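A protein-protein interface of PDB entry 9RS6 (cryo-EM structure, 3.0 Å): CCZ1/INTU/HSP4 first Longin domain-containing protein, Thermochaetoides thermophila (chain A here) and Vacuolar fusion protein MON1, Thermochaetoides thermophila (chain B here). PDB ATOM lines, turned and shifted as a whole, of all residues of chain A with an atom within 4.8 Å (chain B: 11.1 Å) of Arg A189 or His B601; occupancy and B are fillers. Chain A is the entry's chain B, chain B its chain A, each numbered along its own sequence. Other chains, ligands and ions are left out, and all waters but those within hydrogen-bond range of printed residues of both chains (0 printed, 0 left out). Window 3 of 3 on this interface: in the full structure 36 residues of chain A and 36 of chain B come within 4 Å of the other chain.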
ATOM      1  N   SER A 187     -13.831 -25.637  23.444  1.00  0.00           N
ATOM      2  CA  SER A 187     -14.094 -24.960  22.183  1.00  0.00           C
ATOM      3  C   SER A 187     -15.517 -24.425  22.195  1.00  0.00           C
ATOM      4  O   SER A 187     -16.364 -24.875  22.970  1.00  0.00           O
ATOM      5  CB  SER A 187     -13.881 -25.894  20.988  1.00  0.00           C
ATOM      6  OG  SER A 187     -14.218 -25.249  19.774  1.00  0.00           O
ATOM      7  N   SER A 188     -15.773 -23.458  21.319  1.00  0.00           N
ATOM      8  CA  SER A 188     -17.076 -22.808  21.204  1.00  0.00           C
ATOM      9  C   SER A 188     -17.475 -22.671  19.741  1.00  0.00           C
ATOM     10  O   SER A 188     -17.875 -21.601  19.277  1.00  0.00           O
ATOM     11  CB  SER A 188     -17.064 -21.450  21.896  1.00  0.00           C
ATOM     12  OG  SER A 188     -16.147 -20.569  21.273  1.00  0.00           O
ATOM     13  N   ARG A 189     -17.354 -23.768  18.987  1.00  0.00           N
ATOM     14  CA  ARG A 189     -17.675 -23.731  17.562  1.00  0.00           C
ATOM     15  C   ARG A 189     -19.149 -23.427  17.323  1.00  0.00           C
ATOM     16  O   ARG A 189     -19.489 -22.619  16.451  1.00  0.00           O
ATOM     17  CB  ARG A 189     -17.299 -25.059  16.904  1.00  0.00           C
ATOM     18  CG  ARG A 189     -15.820 -25.395  16.957  1.00  0.00           C
ATOM     19  CD  ARG A 189     -15.101 -24.995  15.674  1.00  0.00           C
ATOM     20  NE  ARG A 189     -15.748 -25.527  14.480  1.00  0.00           N
ATOM     21  CZ  ARG A 189     -16.403 -24.790  13.593  1.00  0.00           C
ATOM     22  NH1 ARG A 189     -16.518 -23.480  13.733  1.00  0.00           N
ATOM     23  NH2 ARG A 189     -16.957 -25.383  12.540  1.00  0.00           N
ATOM     24  N   GLU A 190     -20.038 -24.057  18.087  1.00  0.00           N
ATOM     25  CA  GLU A 190     -21.475 -23.916  17.889  1.00  0.00           C
ATOM     26  C   GLU A 190     -22.158 -23.167  19.024  1.00  0.00           C
ATOM     27  O   GLU A 190     -23.386 -23.037  19.016  1.00  0.00           O
ATOM     28  CB  GLU A 190     -22.121 -25.291  17.706  1.00  0.00           C
ATOM     29  CG  GLU A 190     -22.129 -26.151  18.961  1.00  0.00           C
ATOM     30  CD  GLU A 190     -20.897 -27.028  19.081  1.00  0.00           C
ATOM     31  OE1 GLU A 190     -19.848 -26.675  18.502  1.00  0.00           O
ATOM     32  OE2 GLU A 190     -20.977 -28.076  19.757  1.00  0.00           O
ATOM     33  N   VAL A 191     -21.396 -22.678  20.003  1.00  0.00           N
ATOM     34  CA  VAL A 191     -21.979 -21.902  21.089  1.00  0.00           C
ATOM     35  C   VAL A 191     -22.466 -20.567  20.546  1.00  0.00           C
ATOM     36  O   VAL A 191     -21.813 -19.946  19.695  1.00  0.00           O
ATOM     37  CB  VAL A 191     -20.951 -21.709  22.219  1.00  0.00           C
ATOM     38  CG1 VAL A 191     -21.541 -20.893  23.361  1.00  0.00           C
ATOM     39  CG2 VAL A 191     -20.464 -23.053  22.718  1.00  0.00           C
ATOM     40  N   GLN A 555     -21.778 -22.630  10.019  1.00  0.00           N
ATOM     41  CA  GLN A 555     -20.651 -21.773   9.669  1.00  0.00           C
ATOM     42  C   GLN A 555     -21.120 -20.425   9.134  1.00  0.00           C
ATOM     43  O   GLN A 555     -20.773 -19.372   9.689  1.00  0.00           O
ATOM     44  CB  GLN A 555     -19.759 -22.477   8.648  1.00  0.00           C
ATOM     45  CG  GLN A 555     -18.443 -21.769   8.397  1.00  0.00           C
ATOM     46  CD  GLN A 555     -17.643 -21.573   9.669  1.00  0.00           C
ATOM     47  OE1 GLN A 555     -17.574 -20.468  10.207  1.00  0.00           O
ATOM     48  NE2 GLN A 555     -17.035 -22.647  10.157  1.00  0.00           N
ATOM     49  N   ALA A 558     -23.082 -18.347  11.777  1.00  0.00           N
ATOM     50  CA  ALA A 558     -22.178 -17.748  12.743  1.00  0.00           C
ATOM     51  C   ALA A 558     -21.412 -16.574  12.160  1.00  0.00           C
ATOM     52  O   ALA A 558     -21.189 -15.595  12.876  1.00  0.00           O
ATOM     53  CB  ALA A 558     -21.199 -18.796  13.271  1.00  0.00           C
ATOM     54  N   GLN A 559     -21.008 -16.645  10.890  1.00  0.00           N
ATOM     55  CA  GLN A 559     -20.404 -15.481  10.245  1.00  0.00           C
ATOM     56  C   GLN A 559     -21.359 -14.299  10.140  1.00  0.00           C
ATOM     57  O   GLN A 559     -20.938 -13.149  10.328  1.00  0.00           O
ATOM     58  CB  GLN A 559     -19.894 -15.836   8.849  1.00  0.00           C
ATOM     59  CG  GLN A 559     -19.009 -17.052   8.777  1.00  0.00           C
ATOM     60  CD  GLN A 559     -18.602 -17.360   7.359  1.00  0.00           C
ATOM     61  OE1 GLN A 559     -18.777 -16.532   6.470  1.00  0.00           O
ATOM     62  NE2 GLN A 559     -18.060 -18.550   7.137  1.00  0.00           N
ATOM     63  N   LEU B 272      -9.714 -14.794  30.072  1.00  0.00           N
ATOM     64  CA  LEU B 272      -9.124 -14.394  28.803  1.00  0.00           C
ATOM     65  C   LEU B 272      -9.463 -12.961  28.417  1.00  0.00           C
ATOM     66  O   LEU B 272      -9.019 -12.499  27.360  1.00  0.00           O
ATOM     67  CB  LEU B 272      -9.577 -15.338  27.682  1.00  0.00           C
ATOM     68  CG  LEU B 272      -8.766 -16.615  27.448  1.00  0.00           C
ATOM     69  CD1 LEU B 272      -8.972 -17.626  28.566  1.00  0.00           C
ATOM     70  CD2 LEU B 272      -9.123 -17.226  26.102  1.00  0.00           C
ATOM     71  N   SER B 300      -9.585  -6.180  18.415  1.00  0.00           N
ATOM     72  CA  SER B 300     -10.054  -7.517  18.736  1.00  0.00           C
ATOM     73  C   SER B 300      -9.202  -8.151  19.829  1.00  0.00           C
ATOM     74  O   SER B 300      -8.167  -7.622  20.243  1.00  0.00           O
ATOM     75  CB  SER B 300     -10.045  -8.406  17.495  1.00  0.00           C
ATOM     76  OG  SER B 300     -10.236  -9.766  17.842  1.00  0.00           O
ATOM     77  N   ALA B 302      -7.602 -10.952  19.431  1.00  0.00           N
ATOM     78  CA  ALA B 302      -6.404 -11.517  18.818  1.00  0.00           C
ATOM     79  C   ALA B 302      -5.272 -10.498  18.744  1.00  0.00           C
ATOM     80  O   ALA B 302      -4.118 -10.825  19.043  1.00  0.00           O
ATOM     81  CB  ALA B 302      -6.733 -12.053  17.425  1.00  0.00           C
ATOM     82  N   ALA B 595      -9.423  -7.977  12.211  1.00  0.00           N
ATOM     83  CA  ALA B 595     -10.367  -8.636  13.104  1.00  0.00           C
ATOM     84  C   ALA B 595     -11.472  -9.324  12.316  1.00  0.00           C
ATOM     85  O   ALA B 595     -11.912 -10.421  12.676  1.00  0.00           O
ATOM     86  CB  ALA B 595     -10.960  -7.621  14.081  1.00  0.00           C
ATOM     87  N   ALA B 596     -11.937  -8.685  11.240  1.00  0.00           N
ATOM     88  CA  ALA B 596     -12.954  -9.301  10.394  1.00  0.00           C
ATOM     89  C   ALA B 596     -12.434 -10.575   9.736  1.00  0.00           C
ATOM     90  O   ALA B 596     -13.087 -11.623   9.793  1.00  0.00           O
ATOM     91  CB  ALA B 596     -13.433  -8.304   9.341  1.00  0.00           C
ATOM     92  N   LEU B 597     -11.260 -10.505   9.100  1.00  0.00           N
ATOM     93  CA  LEU B 597     -10.726 -11.676   8.408  1.00  0.00           C
ATOM     94  C   LEU B 597     -10.335 -12.773   9.391  1.00  0.00           C
ATOM     95  O   LEU B 597     -10.736 -13.933   9.237  1.00  0.00           O
ATOM     96  CB  LEU B 597      -9.519 -11.297   7.544  1.00  0.00           C
ATOM     97  CG  LEU B 597      -9.724 -10.737   6.130  1.00  0.00           C
ATOM     98  CD1 LEU B 597     -10.559 -11.690   5.285  1.00  0.00           C
ATOM     99  CD2 LEU B 597     -10.293  -9.336   6.108  1.00  0.00           C
ATOM    100  N   HIS B 598      -9.556 -12.425  10.409  1.00  0.00           N
ATOM    101  CA  HIS B 598      -9.028 -13.410  11.353  1.00  0.00           C
ATOM    102  C   HIS B 598      -9.968 -13.581  12.543  1.00  0.00           C
ATOM    103  O   HIS B 598      -9.614 -13.349  13.699  1.00  0.00           O
ATOM    104  CB  HIS B 598      -7.626 -13.010  11.802  1.00  0.00           C
ATOM    105  CG  HIS B 598      -6.565 -13.297  10.787  1.00  0.00           C
ATOM    106  ND1 HIS B 598      -6.588 -12.768   9.516  1.00  0.00           N
ATOM    107  CD2 HIS B 598      -5.449 -14.062  10.857  1.00  0.00           C
ATOM    108  CE1 HIS B 598      -5.533 -13.195   8.845  1.00  0.00           C
ATOM    109  NE2 HIS B 598      -4.825 -13.981   9.637  1.00  0.00           N
ATOM    110  N   ALA B 599     -11.191 -13.999  12.236  1.00  0.00           N
ATOM    111  CA  ALA B 599     -12.195 -14.317  13.241  1.00  0.00           C
ATOM    112  C   ALA B 599     -12.346 -15.830  13.307  1.00  0.00           C
ATOM    113  O   ALA B 599     -12.669 -16.468  12.300  1.00  0.00           O
ATOM    114  CB  ALA B 599     -13.531 -13.650  12.915  1.00  0.00           C
ATOM    115  N   ARG B 600     -12.096 -16.400  14.484  1.00  0.00           N
ATOM    116  CA  ARG B 600     -12.241 -17.837  14.664  1.00  0.00           C
ATOM    117  C   ARG B 600     -13.708 -18.234  14.527  1.00  0.00           C
ATOM    118  O   ARG B 600     -14.614 -17.466  14.863  1.00  0.00           O
ATOM    119  CB  ARG B 600     -11.677 -18.252  16.026  1.00  0.00           C
ATOM    120  CG  ARG B 600     -11.767 -19.736  16.366  1.00  0.00           C
ATOM    121  CD  ARG B 600     -10.825 -20.591  15.519  1.00  0.00           C
ATOM    122  NE  ARG B 600     -11.427 -20.996  14.253  1.00  0.00           N
ATOM    123  CZ  ARG B 600     -10.777 -21.607  13.272  1.00  0.00           C
ATOM    124  NH1 ARG B 600      -9.491 -21.900  13.371  1.00  0.00           N
ATOM    125  NH2 ARG B 600     -11.435 -21.931  12.162  1.00  0.00           N
ATOM    126  N   HIS B 601     -13.932 -19.447  14.007  1.00  0.00           N
ATOM    127  CA  HIS B 601     -15.260 -19.942  13.627  1.00  0.00           C
ATOM    128  C   HIS B 601     -15.904 -19.052  12.570  1.00  0.00           C
ATOM    129  O   HIS B 601     -17.125 -18.875  12.548  1.00  0.00           O
ATOM    130  CB  HIS B 601     -16.192 -20.086  14.836  1.00  0.00           C
ATOM    131  CG  HIS B 601     -15.539 -20.683  16.043  1.00  0.00           C
ATOM    132  ND1 HIS B 601     -14.578 -21.668  15.961  1.00  0.00           N
ATOM    133  CD2 HIS B 601     -15.712 -20.435  17.362  1.00  0.00           C
ATOM    134  CE1 HIS B 601     -14.188 -22.002  17.179  1.00  0.00           C
ATOM    135  NE2 HIS B 601     -14.860 -21.267  18.047  1.00  0.00           N
ATOM    136  N   ALA B 602     -15.082 -18.486  11.686  1.00  0.00           N
ATOM    137  CA  ALA B 602     -15.570 -17.578  10.651  1.00  0.00           C
ATOM    138  C   ALA B 602     -14.553 -17.592   9.512  1.00  0.00           C
ATOM    139  O   ALA B 602     -13.513 -16.934   9.598  1.00  0.00           O
ATOM    140  CB  ALA B 602     -15.772 -16.178  11.213  1.00  0.00           C
ATOM    141  N   HIS B 603     -14.860 -18.343   8.453  1.00  0.00           N
ATOM    142  CA  HIS B 603     -13.949 -18.493   7.316  1.00  0.00           C
ATOM    143  C   HIS B 603     -14.265 -17.438   6.254  1.00  0.00           C
ATOM    144  O   HIS B 603     -14.904 -17.695   5.232  1.00  0.00           O
ATOM    145  CB  HIS B 603     -14.037 -19.904   6.749  1.00  0.00           C
ATOM    146  CG  HIS B 603     -13.557 -20.965   7.690  1.00  0.00           C
ATOM    147  ND1 HIS B 603     -14.386 -21.573   8.608  1.00  0.00           N
ATOM    148  CD2 HIS B 603     -12.337 -21.530   7.853  1.00  0.00           C
ATOM    149  CE1 HIS B 603     -13.697 -22.464   9.299  1.00  0.00           C
ATOM    150  NE2 HIS B 603     -12.451 -22.458   8.859  1.00  0.00           N
ATOM    151  N   LEU B 604     -13.791 -16.222   6.517  1.00  0.00           N
ATOM    152  CA  LEU B 604     -14.004 -15.091   5.619  1.00  0.00           C
ATOM    153  C   LEU B 604     -12.772 -14.915   4.739  1.00  0.00           C
ATOM    154  O   LEU B 604     -11.645 -14.830   5.240  1.00  0.00           O
ATOM    155  CB  LEU B 604     -14.317 -13.819   6.403  1.00  0.00           C
ATOM    156  CG  LEU B 604     -15.756 -13.643   6.906  1.00  0.00           C
ATOM    157  CD1 LEU B 604     -16.098 -14.574   8.047  1.00  0.00           C
ATOM    158  CD2 LEU B 604     -16.008 -12.208   7.320  1.00  0.00           C
ATOM    159  N   ARG B 605     -12.989 -14.870   3.424  1.00  0.00           N
ATOM    160  CA  ARG B 605     -11.879 -14.739   2.487  1.00  0.00           C
ATOM    161  C   ARG B 605     -11.628 -13.279   2.132  1.00  0.00           C
ATOM    162  O   ARG B 605     -10.488 -12.804   2.180  1.00  0.00           O
ATOM    163  CB  ARG B 605     -12.162 -15.564   1.231  1.00  0.00           C
ATOM    164  CG  ARG B 605     -10.994 -15.665   0.268  1.00  0.00           C
ATOM    165  CD  ARG B 605      -9.728 -16.100   0.981  1.00  0.00           C
ATOM    166  NE  ARG B 605      -9.894 -17.346   1.721  1.00  0.00           N
ATOM    167  CZ  ARG B 605      -9.678 -18.552   1.212  1.00  0.00           C
ATOM    168  NH1 ARG B 605      -9.314 -18.715  -0.049  1.00  0.00           N
ATOM    169  NH2 ARG B 605      -9.827 -19.620   1.990  1.00  0.00           N
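O of Ser A188 sits close to NE2 of His B601 (3.3 Å).
ND1 of His B601 sits close to NH1 of Arg A189 (3.5 Å).
The backbone carbonyl oxygen of His B601 sits close to the side-chain amide oxygen of Gln A555, at 2.9 Å.
The side-chain amide nitrogen of Gln A555 sits at hydrogen-bond distance from a ring nitrogen (ND1) of His B603 (3.3 Å).
N of His B603 sits close to NE2 of Gln A559, 3.5 Å away.
A ring nitrogen (NE2) of His B603 sits at hydrogen-bond distance from the guanidinium group (NH2) of Arg B600 (3.5 Å).
Gln A555 touches Ala B602.
Ala B602 touches Gln A559 (CA to CG, 3.95 Å).
Gln A559 touches Leu B604.
Of chain B, only His B601 (3.1 Å) comes within 4 Å of Ser A188.
No residue of chain B comes within 4 Å of Glu A190.
No residue of chain B comes within 4 Å of Val A191.
Of chain B, only His B601, Ala B602 and His B603 come within 4 Å of Gln A555.
No residue of chain B comes within 4 Å of Ala A558.
Ala B595 touches none of the printed residues of chain A.
Of chain A, only Ser A188 (3.1 Å), Arg A189 (3.4 Å) and Gln A555 (2.9 Å) come within 4 Å of His B601.
Printed residues of chain A within 4 Å of Ala B602: Gln A555 and Gln A559.
Of the printed residues of chain A, His B603 touches Gln A555 (3.3 Å) and Gln A559 (3.5 Å).
Of the printed residues of chain A, Leu B604 touches Gln A559.
The nearest printed residue of chain A that does not touch His B601 is Ala A558 (4.1 Å).
Printed residues of chain B that touch a printed residue of chain A: His B601, Ala B602, His B603 and Leu B604.
Hydrophobic or aromatic side chains of chain B within 4 Å of the printed part of chain A: His B601, His B603 and Leu B604.
Among the printed residues, no Asp or Glu carboxylate lies within 4 Å of a Lys or Arg side-chain nitrogen of the other chain.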
